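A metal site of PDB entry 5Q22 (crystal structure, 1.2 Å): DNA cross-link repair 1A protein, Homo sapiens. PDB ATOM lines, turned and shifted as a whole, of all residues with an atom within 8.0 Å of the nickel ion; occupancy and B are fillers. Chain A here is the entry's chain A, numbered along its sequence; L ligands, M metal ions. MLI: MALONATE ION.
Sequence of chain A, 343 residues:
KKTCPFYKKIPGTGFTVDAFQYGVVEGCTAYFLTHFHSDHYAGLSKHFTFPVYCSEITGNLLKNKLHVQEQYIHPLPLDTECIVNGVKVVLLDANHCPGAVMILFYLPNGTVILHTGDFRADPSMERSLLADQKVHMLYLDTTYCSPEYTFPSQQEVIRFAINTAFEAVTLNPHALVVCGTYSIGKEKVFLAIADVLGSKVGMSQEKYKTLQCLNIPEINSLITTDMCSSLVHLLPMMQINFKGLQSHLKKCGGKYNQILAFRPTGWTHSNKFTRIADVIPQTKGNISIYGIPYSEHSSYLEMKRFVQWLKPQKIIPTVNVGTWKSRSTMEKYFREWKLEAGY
Within 4 Å of the nickel ion: His 35, His 37, His 96 and Asp 118.
The nickel ion is bound by O7 of the ligand.
The nickel ion is bound by O9 of the ligand (2.1 Å).
The side-chain carboxylate (OD2) of Asp 118 binds the nickel ion (2.2 Å).
A ring nitrogen (NE2) of His 35 binds the nickel ion.
ND1 of His 37 binds the nickel ion, at 2.3 Å.
A ring nitrogen (NE2) of His 96 binds the nickel ion, 2.3 Å away.
The nickel ion has six donor atoms within binding distance.
OD2 of Asp 118 lies close to NE2 of His 40, at 3.3 Å.
ND1 of His 35 sits at hydrogen-bond distance from OG1 of Thr 34 (2.9 Å).
A ring nitrogen (NE2) of His 37 lies within hydrogen-bond range of the backbone carbonyl oxygen (O) of Ile 184.
ND1 of His 96 is in hydrogen-bond range of O of Glu 296.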
ATOM      1  N   ASP A  18     -10.081 -23.489 -21.891  1.00  0.00           N
ATOM      2  CA  ASP A  18      -9.279 -23.460 -20.636  1.00  0.00           C
ATOM      3  C   ASP A  18     -10.174 -23.245 -19.398  1.00  0.00           C
ATOM      4  O   ASP A  18      -9.865 -22.447 -18.501  1.00  0.00           O
ATOM      5  CB  ASP A  18      -8.170 -22.424 -20.755  1.00  0.00           C
ATOM      6  CG  ASP A  18      -7.195 -22.731 -21.890  1.00  0.00           C
ATOM      7  OD1 ASP A  18      -7.219 -23.861 -22.455  1.00  0.00           O
ATOM      8  OD2 ASP A  18      -6.347 -21.865 -22.196  1.00  0.00           O
ATOM      9  N   THR A  34      -5.857 -25.209 -24.532  1.00  0.00           N
ATOM     10  CA  THR A  34      -4.839 -24.626 -25.422  1.00  0.00           C
ATOM     11  C   THR A  34      -3.410 -25.171 -25.174  1.00  0.00           C
ATOM     12  O   THR A  34      -2.646 -25.292 -26.129  1.00  0.00           O
ATOM     13  CB  THR A  34      -4.810 -23.079 -25.352  1.00  0.00           C
ATOM     14  OG1 THR A  34      -4.424 -22.658 -24.024  1.00  0.00           O
ATOM     15  CG2 THR A  34      -6.147 -22.467 -25.739  1.00  0.00           C
ATOM     16  N   HIS A  35      -3.096 -25.478 -23.912  1.00  0.00           N
ATOM     17  CA  HIS A  35      -1.741 -25.899 -23.547  1.00  0.00           C
ATOM     18  C   HIS A  35      -1.674 -26.454 -22.148  1.00  0.00           C
ATOM     19  O   HIS A  35      -2.524 -26.118 -21.306  1.00  0.00           O
ATOM     20  CB  HIS A  35      -0.672 -24.784 -23.776  1.00  0.00           C
ATOM     21  CG  HIS A  35      -0.722 -23.599 -22.850  1.00  0.00           C
ATOM     22  ND1 HIS A  35      -1.730 -22.657 -22.860  1.00  0.00           N
ATOM     23  CD2 HIS A  35       0.189 -23.147 -21.961  1.00  0.00           C
ATOM     24  CE1 HIS A  35      -1.448 -21.709 -21.972  1.00  0.00           C
ATOM     25  NE2 HIS A  35      -0.282 -21.980 -21.425  1.00  0.00           N
ATOM     26  N   PHE A  36      -0.610 -27.224 -21.881  1.00  0.00           N
ATOM     27  CA  PHE A  36      -0.440 -27.878 -20.572  1.00  0.00           C
ATOM     28  C   PHE A  36       0.338 -27.017 -19.553  1.00  0.00           C
ATOM     29  O   PHE A  36       1.482 -27.352 -19.163  1.00  0.00           O
ATOM     30  CB  PHE A  36       0.242 -29.259 -20.775  1.00  0.00           C
ATOM     31  CG  PHE A  36       0.184 -30.192 -19.564  1.00  0.00           C
ATOM     32  CD1 PHE A  36      -0.994 -30.861 -19.255  1.00  0.00           C
ATOM     33  CD2 PHE A  36       1.296 -30.425 -18.753  1.00  0.00           C
ATOM     34  CE1 PHE A  36      -1.069 -31.733 -18.175  1.00  0.00           C
ATOM     35  CE2 PHE A  36       1.233 -31.304 -17.668  1.00  0.00           C
ATOM     36  CZ  PHE A  36       0.053 -31.956 -17.373  1.00  0.00           C
ATOM     37  N   HIS A  37      -0.264 -25.891 -19.127  1.00  0.00           N
ATOM     38  CA  HIS A  37       0.201 -25.068 -17.992  1.00  0.00           C
ATOM     39  C   HIS A  37      -0.892 -25.073 -16.914  1.00  0.00           C
ATOM     40  O   HIS A  37      -2.089 -24.983 -17.242  1.00  0.00           O
ATOM     41  CB  HIS A  37       0.573 -23.624 -18.400  1.00  0.00           C
ATOM     42  CG  HIS A  37       1.949 -23.491 -19.001  1.00  0.00           C
ATOM     43  ND1 HIS A  37       2.353 -22.376 -19.712  1.00  0.00           N
ATOM     44  CD2 HIS A  37       3.022 -24.316 -18.977  1.00  0.00           C
ATOM     45  CE1 HIS A  37       3.610 -22.521 -20.089  1.00  0.00           C
ATOM     46  NE2 HIS A  37       4.039 -23.690 -19.640  1.00  0.00           N
ATOM     47  N   SER A  38      -0.500 -25.173 -15.635  1.00  0.00           N
ATOM     48  CA  SER A  38      -1.429 -25.448 -14.539  1.00  0.00           C
ATOM     49  C   SER A  38      -2.537 -24.387 -14.375  1.00  0.00           C
ATOM     50  O   SER A  38      -3.652 -24.762 -14.068  1.00  0.00           O
ATOM     51  CB  SER A  38      -0.692 -25.730 -13.217  1.00  0.00           C
ATOM     52  OG  SER A  38      -0.026 -24.581 -12.743  1.00  0.00           O
ATOM     53  N   ASP A  39      -2.276 -23.097 -14.627  1.00  0.00           N
ATOM     54  CA  ASP A  39      -3.367 -22.082 -14.547  1.00  0.00           C
ATOM     55  C   ASP A  39      -4.493 -22.363 -15.584  1.00  0.00           C
ATOM     56  O   ASP A  39      -5.626 -21.919 -15.392  1.00  0.00           O
ATOM     57  CB  ASP A  39      -2.856 -20.636 -14.751  1.00  0.00           C
ATOM     58  CG  ASP A  39      -2.243 -19.997 -13.487  1.00  0.00           C
ATOM     59  OD1 ASP A  39      -2.223 -20.593 -12.385  1.00  0.00           O
ATOM     60  OD2 ASP A  39      -1.772 -18.844 -13.619  1.00  0.00           O
ATOM     61  N   HIS A  40      -4.139 -23.031 -16.709  1.00  0.00           N
ATOM     62  CA  HIS A  40      -5.073 -23.283 -17.805  1.00  0.00           C
ATOM     63  C   HIS A  40      -5.766 -24.639 -17.684  1.00  0.00           C
ATOM     64  O   HIS A  40      -6.993 -24.750 -17.972  1.00  0.00           O
ATOM     65  CB  HIS A  40      -4.336 -23.133 -19.158  1.00  0.00           C
ATOM     66  CG  HIS A  40      -3.848 -21.739 -19.373  1.00  0.00           C
ATOM     67  ND1 HIS A  40      -4.486 -20.835 -20.201  1.00  0.00           N
ATOM     68  CD2 HIS A  40      -2.792 -21.083 -18.827  1.00  0.00           C
ATOM     69  CE1 HIS A  40      -3.854 -19.674 -20.133  1.00  0.00           C
ATOM     70  NE2 HIS A  40      -2.821 -19.803 -19.321  1.00  0.00           N
ATOM     71  N   HIS A  96       4.522 -20.867 -28.029  1.00  0.00           N
ATOM     72  CA  HIS A  96       4.553 -20.743 -26.550  1.00  0.00           C
ATOM     73  C   HIS A  96       5.417 -21.909 -26.056  1.00  0.00           C
ATOM     74  O   HIS A  96       6.629 -21.929 -26.348  1.00  0.00           O
ATOM     75  CB  HIS A  96       3.096 -20.642 -25.988  1.00  0.00           C
ATOM     76  CG  HIS A  96       2.961 -20.424 -24.503  1.00  0.00           C
ATOM     77  ND1 HIS A  96       3.590 -19.389 -23.834  1.00  0.00           N
ATOM     78  CD2 HIS A  96       2.271 -21.107 -23.567  1.00  0.00           C
ATOM     79  CE1 HIS A  96       3.280 -19.457 -22.544  1.00  0.00           C
ATOM     80  NE2 HIS A  96       2.467 -20.481 -22.363  1.00  0.00           N
ATOM     81  N   CYS A  97       4.841 -22.855 -25.330  1.00  0.00           N
ATOM     82  CA  CYS A  97       5.501 -24.080 -24.894  1.00  0.00           C
ATOM     83  C   CYS A  97       5.162 -25.252 -25.852  1.00  0.00           C
ATOM     84  O   CYS A  97       4.263 -25.129 -26.705  1.00  0.00           O
ATOM     85  CB  CYS A  97       5.076 -24.419 -23.443  1.00  0.00           C
ATOM     86  SG  CYS A  97       3.311 -24.795 -23.231  1.00  0.00           S
ATOM     87  N   ALA A 100       1.427 -26.119 -27.431  1.00  0.00           N
ATOM     88  CA  ALA A 100       0.540 -24.958 -27.284  1.00  0.00           C
ATOM     89  C   ALA A 100      -0.048 -24.522 -28.623  1.00  0.00           C
ATOM     90  O   ALA A 100       0.686 -24.403 -29.611  1.00  0.00           O
ATOM     91  CB  ALA A 100       1.241 -23.792 -26.600  1.00  0.00           C
ATOM     92  N   GLY A 117      -4.900 -18.460 -27.001  1.00  0.00           N
ATOM     93  CA  GLY A 117      -4.334 -19.119 -25.818  1.00  0.00           C
ATOM     94  C   GLY A 117      -3.217 -18.216 -25.288  1.00  0.00           C
ATOM     95  O   GLY A 117      -3.329 -16.991 -25.334  1.00  0.00           O
ATOM     96  N   ASP A 118      -2.157 -18.806 -24.751  1.00  0.00           N
ATOM     97  CA  ASP A 118      -0.893 -18.076 -24.499  1.00  0.00           C
ATOM     98  C   ASP A 118      -0.055 -18.156 -25.775  1.00  0.00           C
ATOM     99  O   ASP A 118       0.065 -19.225 -26.387  1.00  0.00           O
ATOM    100  CB  ASP A 118      -0.116 -18.678 -23.319  1.00  0.00           C
ATOM    101  CG  ASP A 118      -0.647 -18.298 -21.944  1.00  0.00           C
ATOM    102  OD1 ASP A 118      -1.529 -17.401 -21.842  1.00  0.00           O
ATOM    103  OD2 ASP A 118      -0.127 -18.873 -20.937  1.00  0.00           O
ATOM    104  N   PHE A 119       0.578 -17.033 -26.179  1.00  0.00           N
ATOM    105  CA  PHE A 119       1.371 -17.026 -27.440  1.00  0.00           C
ATOM    106  C   PHE A 119       2.520 -16.007 -27.363  1.00  0.00           C
ATOM    107  O   PHE A 119       2.451 -15.048 -26.602  1.00  0.00           O
ATOM    108  CB  PHE A 119       0.484 -16.859 -28.709  1.00  0.00           C
ATOM    109  CG  PHE A 119       0.123 -15.423 -29.143  1.00  0.00           C
ATOM    110  CD1 PHE A 119       0.109 -15.088 -30.502  1.00  0.00           C
ATOM    111  CD2 PHE A 119      -0.257 -14.432 -28.243  1.00  0.00           C
ATOM    112  CE1 PHE A 119      -0.281 -13.836 -30.961  1.00  0.00           C
ATOM    113  CE2 PHE A 119      -0.638 -13.161 -28.680  1.00  0.00           C
ATOM    114  CZ  PHE A 119      -0.650 -12.867 -30.033  1.00  0.00           C
ATOM    115  N   ASP A 141      -3.963 -12.966 -25.619  1.00  0.00           N
ATOM    116  CA  ASP A 141      -2.965 -13.052 -24.496  1.00  0.00           C
ATOM    117  C   ASP A 141      -2.277 -11.691 -24.364  1.00  0.00           C
ATOM    118  O   ASP A 141      -1.377 -11.360 -25.149  1.00  0.00           O
ATOM    119  CB  ASP A 141      -1.946 -14.160 -24.755  1.00  0.00           C
ATOM    120  CG  ASP A 141      -0.739 -14.127 -23.826  1.00  0.00           C
ATOM    121  OD1 ASP A 141      -0.843 -13.428 -22.772  1.00  0.00           O
ATOM    122  OD2 ASP A 141       0.260 -14.824 -24.163  1.00  0.00           O
ATOM    123  N   THR A 143      -0.564 -10.577 -21.622  1.00  0.00           N
ATOM    124  CA  THR A 143       0.386 -10.653 -20.494  1.00  0.00           C
ATOM    125  C   THR A 143       1.275  -9.413 -20.386  1.00  0.00           C
ATOM    126  O   THR A 143       1.328  -8.780 -19.304  1.00  0.00           O
ATOM    127  CB  THR A 143       1.258 -11.944 -20.585  1.00  0.00           C
ATOM    128  OG1 THR A 143       0.430 -13.111 -20.450  1.00  0.00           O
ATOM    129  CG2 THR A 143       2.301 -12.029 -19.468  1.00  0.00           C
ATOM    130  N   SER A 183       7.698 -26.064 -14.979  1.00  0.00           N
ATOM    131  CA  SER A 183       6.634 -26.299 -15.939  1.00  0.00           C
ATOM    132  C   SER A 183       7.290 -26.698 -17.271  1.00  0.00           C
ATOM    133  O   SER A 183       8.526 -26.565 -17.440  1.00  0.00           O
ATOM    134  CB  SER A 183       5.770 -25.037 -16.161  1.00  0.00           C
ATOM    135  OG  SER A 183       6.554 -23.965 -16.689  1.00  0.00           O
ATOM    136  N   ILE A 184       6.497 -27.163 -18.215  1.00  0.00           N
ATOM    137  CA  ILE A 184       7.003 -27.282 -19.583  1.00  0.00           C
ATOM    138  C   ILE A 184       7.215 -25.878 -20.197  1.00  0.00           C
ATOM    139  O   ILE A 184       6.678 -24.859 -19.714  1.00  0.00           O
ATOM    140  CB  ILE A 184       6.110 -28.182 -20.496  1.00  0.00           C
ATOM    141  CG1 ILE A 184       4.744 -27.565 -20.787  1.00  0.00           C
ATOM    142  CG2 ILE A 184       6.004 -29.585 -19.912  1.00  0.00           C
ATOM    143  CD1 ILE A 184       4.007 -28.278 -21.900  1.00  0.00           C
ATOM    144  N   GLU A 296       8.320 -16.733 -23.329  1.00  0.00           N
ATOM    145  CA  GLU A 296       7.387 -17.429 -24.232  1.00  0.00           C
ATOM    146  C   GLU A 296       6.038 -16.680 -24.388  1.00  0.00           C
ATOM    147  O   GLU A 296       5.029 -17.259 -24.844  1.00  0.00           O
ATOM    148  CB  GLU A 296       7.234 -18.922 -23.840  1.00  0.00           C
ATOM    149  CG  GLU A 296       8.533 -19.720 -24.150  1.00  0.00           C
ATOM    150  CD  GLU A 296       8.487 -21.233 -23.965  1.00  0.00           C
ATOM    151  OE1 GLU A 296       7.592 -21.717 -23.209  1.00  0.00           O
ATOM    152  OE2 GLU A 296       9.397 -21.941 -24.563  1.00  0.00           O
ATOM    153  N   HIS A 297       6.033 -15.385 -24.037  1.00  0.00           N
ATOM    154  CA  HIS A 297       4.905 -14.493 -24.344  1.00  0.00           C
ATOM    155  C   HIS A 297       5.373 -13.313 -25.213  1.00  0.00           C
ATOM    156  O   HIS A 297       6.541 -12.863 -25.132  1.00  0.00           O
ATOM    157  CB  HIS A 297       4.281 -13.895 -23.063  1.00  0.00           C
ATOM    158  CG  HIS A 297       3.600 -14.870 -22.155  1.00  0.00           C
ATOM    159  ND1 HIS A 297       2.299 -15.288 -22.305  1.00  0.00           N
ATOM    160  CD2 HIS A 297       4.065 -15.499 -21.041  1.00  0.00           C
ATOM    161  CE1 HIS A 297       1.985 -16.113 -21.331  1.00  0.00           C
ATOM    162  NE2 HIS A 297       3.053 -16.274 -20.567  1.00  0.00           N
HETATM  163  C1  MLI L   1       2.172 -19.665 -17.354  1.00  0.00           C
HETATM  164  C2  MLI L   1       2.776 -18.845 -18.466  1.00  0.00           C
HETATM  165  C3  MLI L   1       0.655 -19.899 -17.506  1.00  0.00           C
HETATM  166  O6  MLI L   1       3.499 -17.856 -18.237  1.00  0.00           O
HETATM  167  O7  MLI L   1       2.542 -19.206 -19.625  1.00  0.00           O
HETATM  168  O8  MLI L   1      -0.085 -19.639 -16.532  1.00  0.00           O
HETATM  169  O9  MLI L   1       0.205 -20.412 -18.565  1.00  0.00           O
HETATM  170 NI    NI M   1       1.173 -20.578 -20.444  1.00  0.00          NI
